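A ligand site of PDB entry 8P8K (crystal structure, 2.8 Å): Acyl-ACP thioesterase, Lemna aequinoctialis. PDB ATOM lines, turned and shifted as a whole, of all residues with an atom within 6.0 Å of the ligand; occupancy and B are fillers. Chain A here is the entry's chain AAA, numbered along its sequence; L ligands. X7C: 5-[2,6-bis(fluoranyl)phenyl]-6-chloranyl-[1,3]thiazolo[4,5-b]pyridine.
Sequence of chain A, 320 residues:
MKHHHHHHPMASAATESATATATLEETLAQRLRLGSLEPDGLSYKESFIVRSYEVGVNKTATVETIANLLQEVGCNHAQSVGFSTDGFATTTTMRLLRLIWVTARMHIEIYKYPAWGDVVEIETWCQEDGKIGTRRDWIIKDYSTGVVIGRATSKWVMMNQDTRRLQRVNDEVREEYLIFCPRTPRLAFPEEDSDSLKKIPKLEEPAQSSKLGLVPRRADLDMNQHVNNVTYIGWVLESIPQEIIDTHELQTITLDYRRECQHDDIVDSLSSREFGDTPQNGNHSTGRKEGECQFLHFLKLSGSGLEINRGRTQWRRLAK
N12 of the ligand lies within hydrogen-bond range of NE of Arg 136. OG1 of Thr 134 lies close to S14 of the ligand, at 3.3 Å. N10 of the ligand sits at hydrogen-bond distance from SG of Cys 126.
NH2 of Arg 136 sits at hydrogen-bond distance from ND1 of His 77 (3.1 Å). The side-chain sulfur of Cys 181 sits at hydrogen-bond distance from the backbone carbonyl oxygen of Tyr 177 (3.7 Å). O of Cys 126 is in hydrogen-bond range of SG of Cys 181 (3.0 Å). The backbone carbonyl oxygen of Ala 78 lies close to the backbone NH of Phe 83 (3.3 Å). The backbone carbonyl oxygen (O) of Thr 134 sits at hydrogen-bond distance from the backbone NH (N) of Trp 156 (2.7 Å). SD of Met 94 lies within hydrogen-bond range of NE1 of Trp 101, at 3.3 Å. O of Arg 135 lies close to SG of Cys 126, at 3.5 Å. The side-chain hydroxyl (OG) of Ser 154 lies within hydrogen-bond range of the indole nitrogen (NE1) of Trp 156 (2.7 Å).
A fluorine (F1) of the ligand sits close to the side-chain sulfur of Cys 181 (3.3 Å). NE2 of His 77 touches C4 of the ligand (3.3 Å). Ala 78 touches the ligand. CG2 of Val 81 touches C5 of the ligand, at 3.7 Å. Phe 83 touches the ligand (CE2 to C5, 3.6 Å). CZ of Phe 88 touches N12 of the ligand, 3.2 Å away. Ala 89 touches the ligand (CB to F7, 3.4 Å). Trp 101 touches the ligand (NE1 to C16, 3.3 Å). CG of Trp 156 touches S14 of the ligand (3.5 Å). Tyr 177 touches the ligand. Phe 180 touches the ligand.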
ATOM      1  N   GLY A  74      24.325  28.400  11.806  1.00  0.00           N
ATOM      2  CA  GLY A  74      22.956  28.308  12.353  1.00  0.00           C
ATOM      3  C   GLY A  74      22.868  27.312  13.506  1.00  0.00           C
ATOM      4  O   GLY A  74      22.229  27.623  14.554  1.00  0.00           O
ATOM      5  N   CYS A  75      23.485  26.140  13.370  1.00  0.00           N
ATOM      6  CA  CYS A  75      23.464  25.114  14.438  1.00  0.00           C
ATOM      7  C   CYS A  75      24.221  25.669  15.663  1.00  0.00           C
ATOM      8  O   CYS A  75      23.765  25.451  16.783  1.00  0.00           O
ATOM      9  CB  CYS A  75      24.028  23.776  13.960  1.00  0.00           C
ATOM     10  SG  CYS A  75      22.924  22.919  12.801  1.00  0.00           S
ATOM     11  N   HIS A  77      24.685  28.808  16.543  1.00  0.00           N
ATOM     12  CA  HIS A  77      23.806  29.850  17.147  1.00  0.00           C
ATOM     13  C   HIS A  77      22.801  29.154  18.072  1.00  0.00           C
ATOM     14  O   HIS A  77      22.710  29.531  19.243  1.00  0.00           O
ATOM     15  CB  HIS A  77      23.163  30.703  16.045  1.00  0.00           C
ATOM     16  CG  HIS A  77      22.173  31.687  16.543  1.00  0.00           C
ATOM     17  ND1 HIS A  77      21.238  32.289  15.715  1.00  0.00           N
ATOM     18  CD2 HIS A  77      21.932  32.192  17.780  1.00  0.00           C
ATOM     19  CE1 HIS A  77      20.475  33.101  16.414  1.00  0.00           C
ATOM     20  NE2 HIS A  77      20.880  33.050  17.682  1.00  0.00           N
ATOM     21  N   ALA A  78      22.096  28.127  17.586  1.00  0.00           N
ATOM     22  CA  ALA A  78      21.204  27.303  18.438  1.00  0.00           C
ATOM     23  C   ALA A  78      21.960  26.843  19.702  1.00  0.00           C
ATOM     24  O   ALA A  78      21.524  27.116  20.830  1.00  0.00           O
ATOM     25  CB  ALA A  78      20.696  26.121  17.660  1.00  0.00           C
ATOM     26  N   GLN A  79      23.076  26.150  19.524  1.00  0.00           N
ATOM     27  CA  GLN A  79      23.844  25.607  20.672  1.00  0.00           C
ATOM     28  C   GLN A  79      24.125  26.768  21.626  1.00  0.00           C
ATOM     29  O   GLN A  79      24.066  26.540  22.831  1.00  0.00           O
ATOM     30  CB  GLN A  79      25.100  24.897  20.160  1.00  0.00           C
ATOM     31  CG  GLN A  79      26.100  24.521  21.245  1.00  0.00           C
ATOM     32  CD  GLN A  79      27.347  23.822  20.736  1.00  0.00           C
ATOM     33  OE1 GLN A  79      28.395  23.881  21.381  1.00  0.00           O
ATOM     34  NE2 GLN A  79      27.271  23.150  19.601  1.00  0.00           N
ATOM     35  N   VAL A  81      22.554  29.456  22.520  1.00  0.00           N
ATOM     36  CA  VAL A  81      21.455  30.008  23.379  1.00  0.00           C
ATOM     37  C   VAL A  81      20.801  28.883  24.190  1.00  0.00           C
ATOM     38  O   VAL A  81      19.776  29.149  24.837  1.00  0.00           O
ATOM     39  CB  VAL A  81      20.438  30.817  22.552  1.00  0.00           C
ATOM     40  CG1 VAL A  81      21.103  32.026  21.917  1.00  0.00           C
ATOM     41  CG2 VAL A  81      19.738  29.963  21.512  1.00  0.00           C
ATOM     42  N   PHE A  83      19.933  25.538  23.252  1.00  0.00           N
ATOM     43  CA  PHE A  83      19.360  24.348  22.562  1.00  0.00           C
ATOM     44  C   PHE A  83      20.347  23.198  22.804  1.00  0.00           C
ATOM     45  O   PHE A  83      21.547  23.449  23.032  1.00  0.00           O
ATOM     46  CB  PHE A  83      19.100  24.641  21.078  1.00  0.00           C
ATOM     47  CG  PHE A  83      18.002  25.649  20.844  1.00  0.00           C
ATOM     48  CD1 PHE A  83      16.677  25.316  21.053  1.00  0.00           C
ATOM     49  CD2 PHE A  83      18.291  26.940  20.414  1.00  0.00           C
ATOM     50  CE1 PHE A  83      15.677  26.254  20.846  1.00  0.00           C
ATOM     51  CE2 PHE A  83      17.283  27.872  20.205  1.00  0.00           C
ATOM     52  CZ  PHE A  83      15.974  27.531  20.426  1.00  0.00           C
ATOM     53  N   PHE A  88      18.427  20.409  15.574  1.00  0.00           N
ATOM     54  CA  PHE A  88      18.763  21.803  15.212  1.00  0.00           C
ATOM     55  C   PHE A  88      17.641  22.737  15.675  1.00  0.00           C
ATOM     56  O   PHE A  88      16.598  22.796  15.001  1.00  0.00           O
ATOM     57  CB  PHE A  88      18.973  21.969  13.716  1.00  0.00           C
ATOM     58  CG  PHE A  88      19.023  23.407  13.278  1.00  0.00           C
ATOM     59  CD1 PHE A  88      19.593  24.381  14.092  1.00  0.00           C
ATOM     60  CD2 PHE A  88      18.513  23.802  12.056  1.00  0.00           C
ATOM     61  CE1 PHE A  88      19.646  25.706  13.685  1.00  0.00           C
ATOM     62  CE2 PHE A  88      18.599  25.118  11.645  1.00  0.00           C
ATOM     63  CZ  PHE A  88      19.161  26.069  12.451  1.00  0.00           C
ATOM     64  N   ALA A  89      17.902  23.464  16.765  1.00  0.00           N
ATOM     65  CA  ALA A  89      17.042  24.549  17.316  1.00  0.00           C
ATOM     66  C   ALA A  89      15.694  23.965  17.734  1.00  0.00           C
ATOM     67  O   ALA A  89      14.687  24.682  17.627  1.00  0.00           O
ATOM     68  CB  ALA A  89      16.862  25.653  16.307  1.00  0.00           C
ATOM     69  N   THR A  91      13.247  23.049  20.533  1.00  0.00           N
ATOM     70  CA  THR A  91      13.036  23.521  21.914  1.00  0.00           C
ATOM     71  C   THR A  91      12.637  22.319  22.762  1.00  0.00           C
ATOM     72  O   THR A  91      12.290  21.246  22.201  1.00  0.00           O
ATOM     73  CB  THR A  91      12.032  24.680  22.001  1.00  0.00           C
ATOM     74  OG1 THR A  91      10.705  24.160  22.054  1.00  0.00           O
ATOM     75  CG2 THR A  91      12.145  25.673  20.862  1.00  0.00           C
ATOM     76  N   MET A  94       9.473  20.806  21.513  1.00  0.00           N
ATOM     77  CA  MET A  94       9.719  20.148  20.206  1.00  0.00           C
ATOM     78  C   MET A  94      10.343  18.780  20.475  1.00  0.00           C
ATOM     79  O   MET A  94       9.935  17.773  19.847  1.00  0.00           O
ATOM     80  CB  MET A  94      10.654  21.004  19.340  1.00  0.00           C
ATOM     81  CG  MET A  94      10.033  22.317  18.905  1.00  0.00           C
ATOM     82  SD  MET A  94      11.033  23.246  17.728  1.00  0.00           S
ATOM     83  CE  MET A  94      11.199  22.059  16.408  1.00  0.00           C
ATOM     84  N   TRP A 101      12.831  21.104  12.727  1.00  0.00           N
ATOM     85  CA  TRP A 101      12.689  22.188  11.733  1.00  0.00           C
ATOM     86  C   TRP A 101      13.164  21.679  10.380  1.00  0.00           C
ATOM     87  O   TRP A 101      14.215  21.034  10.330  1.00  0.00           O
ATOM     88  CB  TRP A 101      13.498  23.402  12.144  1.00  0.00           C
ATOM     89  CG  TRP A 101      13.009  24.081  13.382  1.00  0.00           C
ATOM     90  CD1 TRP A 101      13.592  24.059  14.611  1.00  0.00           C
ATOM     91  CD2 TRP A 101      11.864  24.930  13.499  1.00  0.00           C
ATOM     92  NE1 TRP A 101      12.888  24.844  15.479  1.00  0.00           N
ATOM     93  CE2 TRP A 101      11.810  25.381  14.825  1.00  0.00           C
ATOM     94  CE3 TRP A 101      10.869  25.360  12.608  1.00  0.00           C
ATOM     95  CZ2 TRP A 101      10.827  26.250  15.287  1.00  0.00           C
ATOM     96  CZ3 TRP A 101       9.887  26.213  13.065  1.00  0.00           C
ATOM     97  CH2 TRP A 101       9.870  26.651  14.379  1.00  0.00           C
ATOM     98  N   CYS A 126      17.560  34.741  13.662  1.00  0.00           N
ATOM     99  CA  CYS A 126      16.280  34.099  13.347  1.00  0.00           C
ATOM    100  C   CYS A 126      15.141  34.979  13.845  1.00  0.00           C
ATOM    101  O   CYS A 126      15.118  35.333  15.021  1.00  0.00           O
ATOM    102  CB  CYS A 126      16.251  32.714  13.965  1.00  0.00           C
ATOM    103  SG  CYS A 126      14.808  31.791  13.400  1.00  0.00           S
ATOM    104  N   GLN A 127      14.241  35.337  12.945  1.00  0.00           N
ATOM    105  CA  GLN A 127      13.020  36.082  13.297  1.00  0.00           C
ATOM    106  C   GLN A 127      11.821  35.247  12.882  1.00  0.00           C
ATOM    107  O   GLN A 127      11.990  34.232  12.218  1.00  0.00           O
ATOM    108  CB  GLN A 127      13.041  37.462  12.678  1.00  0.00           C
ATOM    109  CG  GLN A 127      13.892  38.438  13.479  1.00  0.00           C
ATOM    110  CD  GLN A 127      13.824  39.801  12.856  1.00  0.00           C
ATOM    111  OE1 GLN A 127      14.205  39.993  11.707  1.00  0.00           O
ATOM    112  NE2 GLN A 127      13.303  40.751  13.602  1.00  0.00           N
ATOM    113  N   THR A 134       9.459  30.071  10.873  1.00  0.00           N
ATOM    114  CA  THR A 134      10.603  30.940  11.248  1.00  0.00           C
ATOM    115  C   THR A 134      11.451  31.249  10.009  1.00  0.00           C
ATOM    116  O   THR A 134      11.574  30.393   9.123  1.00  0.00           O
ATOM    117  CB  THR A 134      11.389  30.304  12.403  1.00  0.00           C
ATOM    118  OG1 THR A 134      12.162  29.185  11.962  1.00  0.00           O
ATOM    119  CG2 THR A 134      10.506  29.825  13.522  1.00  0.00           C
ATOM    120  N   ARG A 135      12.065  32.421  10.009  1.00  0.00           N
ATOM    121  CA  ARG A 135      12.991  32.879   8.942  1.00  0.00           C
ATOM    122  C   ARG A 135      14.412  32.988   9.521  1.00  0.00           C
ATOM    123  O   ARG A 135      14.584  33.760  10.456  1.00  0.00           O
ATOM    124  CB  ARG A 135      12.479  34.210   8.414  1.00  0.00           C
ATOM    125  CG  ARG A 135      13.277  34.754   7.228  1.00  0.00           C
ATOM    126  CD  ARG A 135      12.828  36.132   6.773  1.00  0.00           C
ATOM    127  NE  ARG A 135      13.580  37.191   7.448  1.00  0.00           N
ATOM    128  CZ  ARG A 135      13.093  37.988   8.396  1.00  0.00           C
ATOM    129  NH1 ARG A 135      11.828  37.876   8.779  1.00  0.00           N
ATOM    130  NH2 ARG A 135      13.863  38.885   8.974  1.00  0.00           N
ATOM    131  N   ARG A 136      15.395  32.258   8.985  1.00  0.00           N
ATOM    132  CA  ARG A 136      16.820  32.437   9.364  1.00  0.00           C
ATOM    133  C   ARG A 136      17.540  33.184   8.231  1.00  0.00           C
ATOM    134  O   ARG A 136      17.382  32.792   7.083  1.00  0.00           O
ATOM    135  CB  ARG A 136      17.535  31.115   9.639  1.00  0.00           C
ATOM    136  CG  ARG A 136      18.998  31.282  10.006  1.00  0.00           C
ATOM    137  CD  ARG A 136      19.591  30.035  10.626  1.00  0.00           C
ATOM    138  NE  ARG A 136      19.181  29.930  12.012  1.00  0.00           N
ATOM    139  CZ  ARG A 136      19.794  30.516  13.035  1.00  0.00           C
ATOM    140  NH1 ARG A 136      20.888  31.236  12.829  1.00  0.00           N
ATOM    141  NH2 ARG A 136      19.338  30.348  14.267  1.00  0.00           N
ATOM    142  N   SER A 154      15.857  32.206   4.496  1.00  0.00           N
ATOM    143  CA  SER A 154      15.239  30.870   4.495  1.00  0.00           C
ATOM    144  C   SER A 154      13.957  30.924   5.302  1.00  0.00           C
ATOM    145  O   SER A 154      13.853  31.730   6.216  1.00  0.00           O
ATOM    146  CB  SER A 154      16.199  29.851   5.040  1.00  0.00           C
ATOM    147  OG  SER A 154      16.562  30.171   6.376  1.00  0.00           O
ATOM    148  N   TRP A 156      11.618  28.215   7.501  1.00  0.00           N
ATOM    149  CA  TRP A 156      11.562  26.877   8.135  1.00  0.00           C
ATOM    150  C   TRP A 156      10.188  26.675   8.743  1.00  0.00           C
ATOM    151  O   TRP A 156       9.538  27.659   9.154  1.00  0.00           O
ATOM    152  CB  TRP A 156      12.689  26.703   9.164  1.00  0.00           C
ATOM    153  CG  TRP A 156      14.070  26.927   8.622  1.00  0.00           C
ATOM    154  CD1 TRP A 156      14.590  28.097   8.141  1.00  0.00           C
ATOM    155  CD2 TRP A 156      15.121  25.947   8.517  1.00  0.00           C
ATOM    156  NE1 TRP A 156      15.881  27.913   7.737  1.00  0.00           N
ATOM    157  CE2 TRP A 156      16.235  26.613   7.952  1.00  0.00           C
ATOM    158  CE3 TRP A 156      15.234  24.586   8.821  1.00  0.00           C
ATOM    159  CZ2 TRP A 156      17.439  25.959   7.711  1.00  0.00           C
ATOM    160  CZ3 TRP A 156      16.436  23.948   8.585  1.00  0.00           C
ATOM    161  CH2 TRP A 156      17.517  24.623   8.023  1.00  0.00           C
ATOM    162  N   TYR A 177      11.351  30.173  22.099  1.00  0.00           N
ATOM    163  CA  TYR A 177      12.415  30.645  21.168  1.00  0.00           C
ATOM    164  C   TYR A 177      12.359  32.168  20.974  1.00  0.00           C
ATOM    165  O   TYR A 177      13.374  32.775  20.592  1.00  0.00           O
ATOM    166  CB  TYR A 177      12.370  29.853  19.845  1.00  0.00           C
ATOM    167  CG  TYR A 177      11.239  30.101  18.870  1.00  0.00           C
ATOM    168  CD1 TYR A 177      11.064  31.335  18.252  1.00  0.00           C
ATOM    169  CD2 TYR A 177      10.399  29.072  18.481  1.00  0.00           C
ATOM    170  CE1 TYR A 177      10.057  31.541  17.320  1.00  0.00           C
ATOM    171  CE2 TYR A 177       9.377  29.261  17.559  1.00  0.00           C
ATOM    172  CZ  TYR A 177       9.206  30.500  16.965  1.00  0.00           C
ATOM    173  OH  TYR A 177       8.204  30.697  16.038  1.00  0.00           O
ATOM    174  N   LEU A 178      11.211  32.780  21.223  1.00  0.00           N
ATOM    175  CA  LEU A 178      10.958  34.150  20.717  1.00  0.00           C
ATOM    176  C   LEU A 178      11.850  35.140  21.463  1.00  0.00           C
ATOM    177  O   LEU A 178      12.084  36.244  20.944  1.00  0.00           O
ATOM    178  CB  LEU A 178       9.483  34.491  20.900  1.00  0.00           C
ATOM    179  CG  LEU A 178       8.834  35.088  19.663  1.00  0.00           C
ATOM    180  CD1 LEU A 178       7.348  35.317  19.929  1.00  0.00           C
ATOM    181  CD2 LEU A 178       9.539  36.379  19.254  1.00  0.00           C
ATOM    182  N   PHE A 180      14.900  34.939  21.807  1.00  0.00           N
ATOM    183  CA  PHE A 180      16.219  34.971  21.116  1.00  0.00           C
ATOM    184  C   PHE A 180      16.078  35.479  19.684  1.00  0.00           C
ATOM    185  O   PHE A 180      17.050  35.353  18.912  1.00  0.00           O
ATOM    186  CB  PHE A 180      16.844  33.576  21.183  1.00  0.00           C
ATOM    187  CG  PHE A 180      17.067  33.071  22.584  1.00  0.00           C
ATOM    188  CD1 PHE A 180      17.916  33.748  23.446  1.00  0.00           C
ATOM    189  CD2 PHE A 180      16.452  31.918  23.035  1.00  0.00           C
ATOM    190  CE1 PHE A 180      18.148  33.280  24.732  1.00  0.00           C
ATOM    191  CE2 PHE A 180      16.668  31.455  24.323  1.00  0.00           C
ATOM    192  CZ  PHE A 180      17.516  32.136  25.172  1.00  0.00           C
ATOM    193  N   CYS A 181      14.925  36.023  19.332  1.00  0.00           N
ATOM    194  CA  CYS A 181      14.671  36.646  18.014  1.00  0.00           C
ATOM    195  C   CYS A 181      14.558  38.158  18.220  1.00  0.00           C
ATOM    196  O   CYS A 181      13.854  38.604  19.104  1.00  0.00           O
ATOM    197  CB  CYS A 181      13.386  36.099  17.403  1.00  0.00           C
ATOM    198  SG  CYS A 181      13.389  34.298  17.189  1.00  0.00           S
HETATM  199  C2  X7C L   1      16.151  31.040  17.240  1.00  0.00           C
HETATM  200  C4  X7C L   1      18.099  31.452  18.538  1.00  0.00           C
HETATM  201  C5  X7C L   1      18.691  30.338  18.028  1.00  0.00           C
HETATM  202  C6  X7C L   1      18.023  29.586  17.131  1.00  0.00           C
HETATM  203  C8  X7C L   1      16.738  29.883  16.731  1.00  0.00           C
HETATM  204  C9  X7C L   1      16.056  29.075  15.683  1.00  0.00           C
HETATM  205  C11 X7C L   1      16.257  28.407  13.474  1.00  0.00           C
HETATM  206  C13 X7C L   1      16.155  27.601  11.435  1.00  0.00           C
HETATM  207  C15 X7C L   1      15.011  27.756  13.557  1.00  0.00           C
HETATM  208  C16 X7C L   1      14.279  27.772  14.713  1.00  0.00           C
HETATM  209  C17 X7C L   1      14.788  28.448  15.781  1.00  0.00           C
HETATM  210  F1  X7C L   1      14.913  31.431  16.878  1.00  0.00           F
HETATM  211  C3  X7C L   1      16.826  31.814  18.144  1.00  0.00           C
HETATM  212  F7  X7C L   1      18.649  28.518  16.657  1.00  0.00           F
HETATM  213  N10 X7C L   1      16.719  29.047  14.532  1.00  0.00           N
HETATM  214  N12 X7C L   1      16.811  28.284  12.280  1.00  0.00           N
HETATM  215  S14 X7C L   1      14.661  27.006  12.030  1.00  0.00           S
HETATM  216 CL18 X7C L   1      13.784  28.369  17.165  1.00  0.00          CL
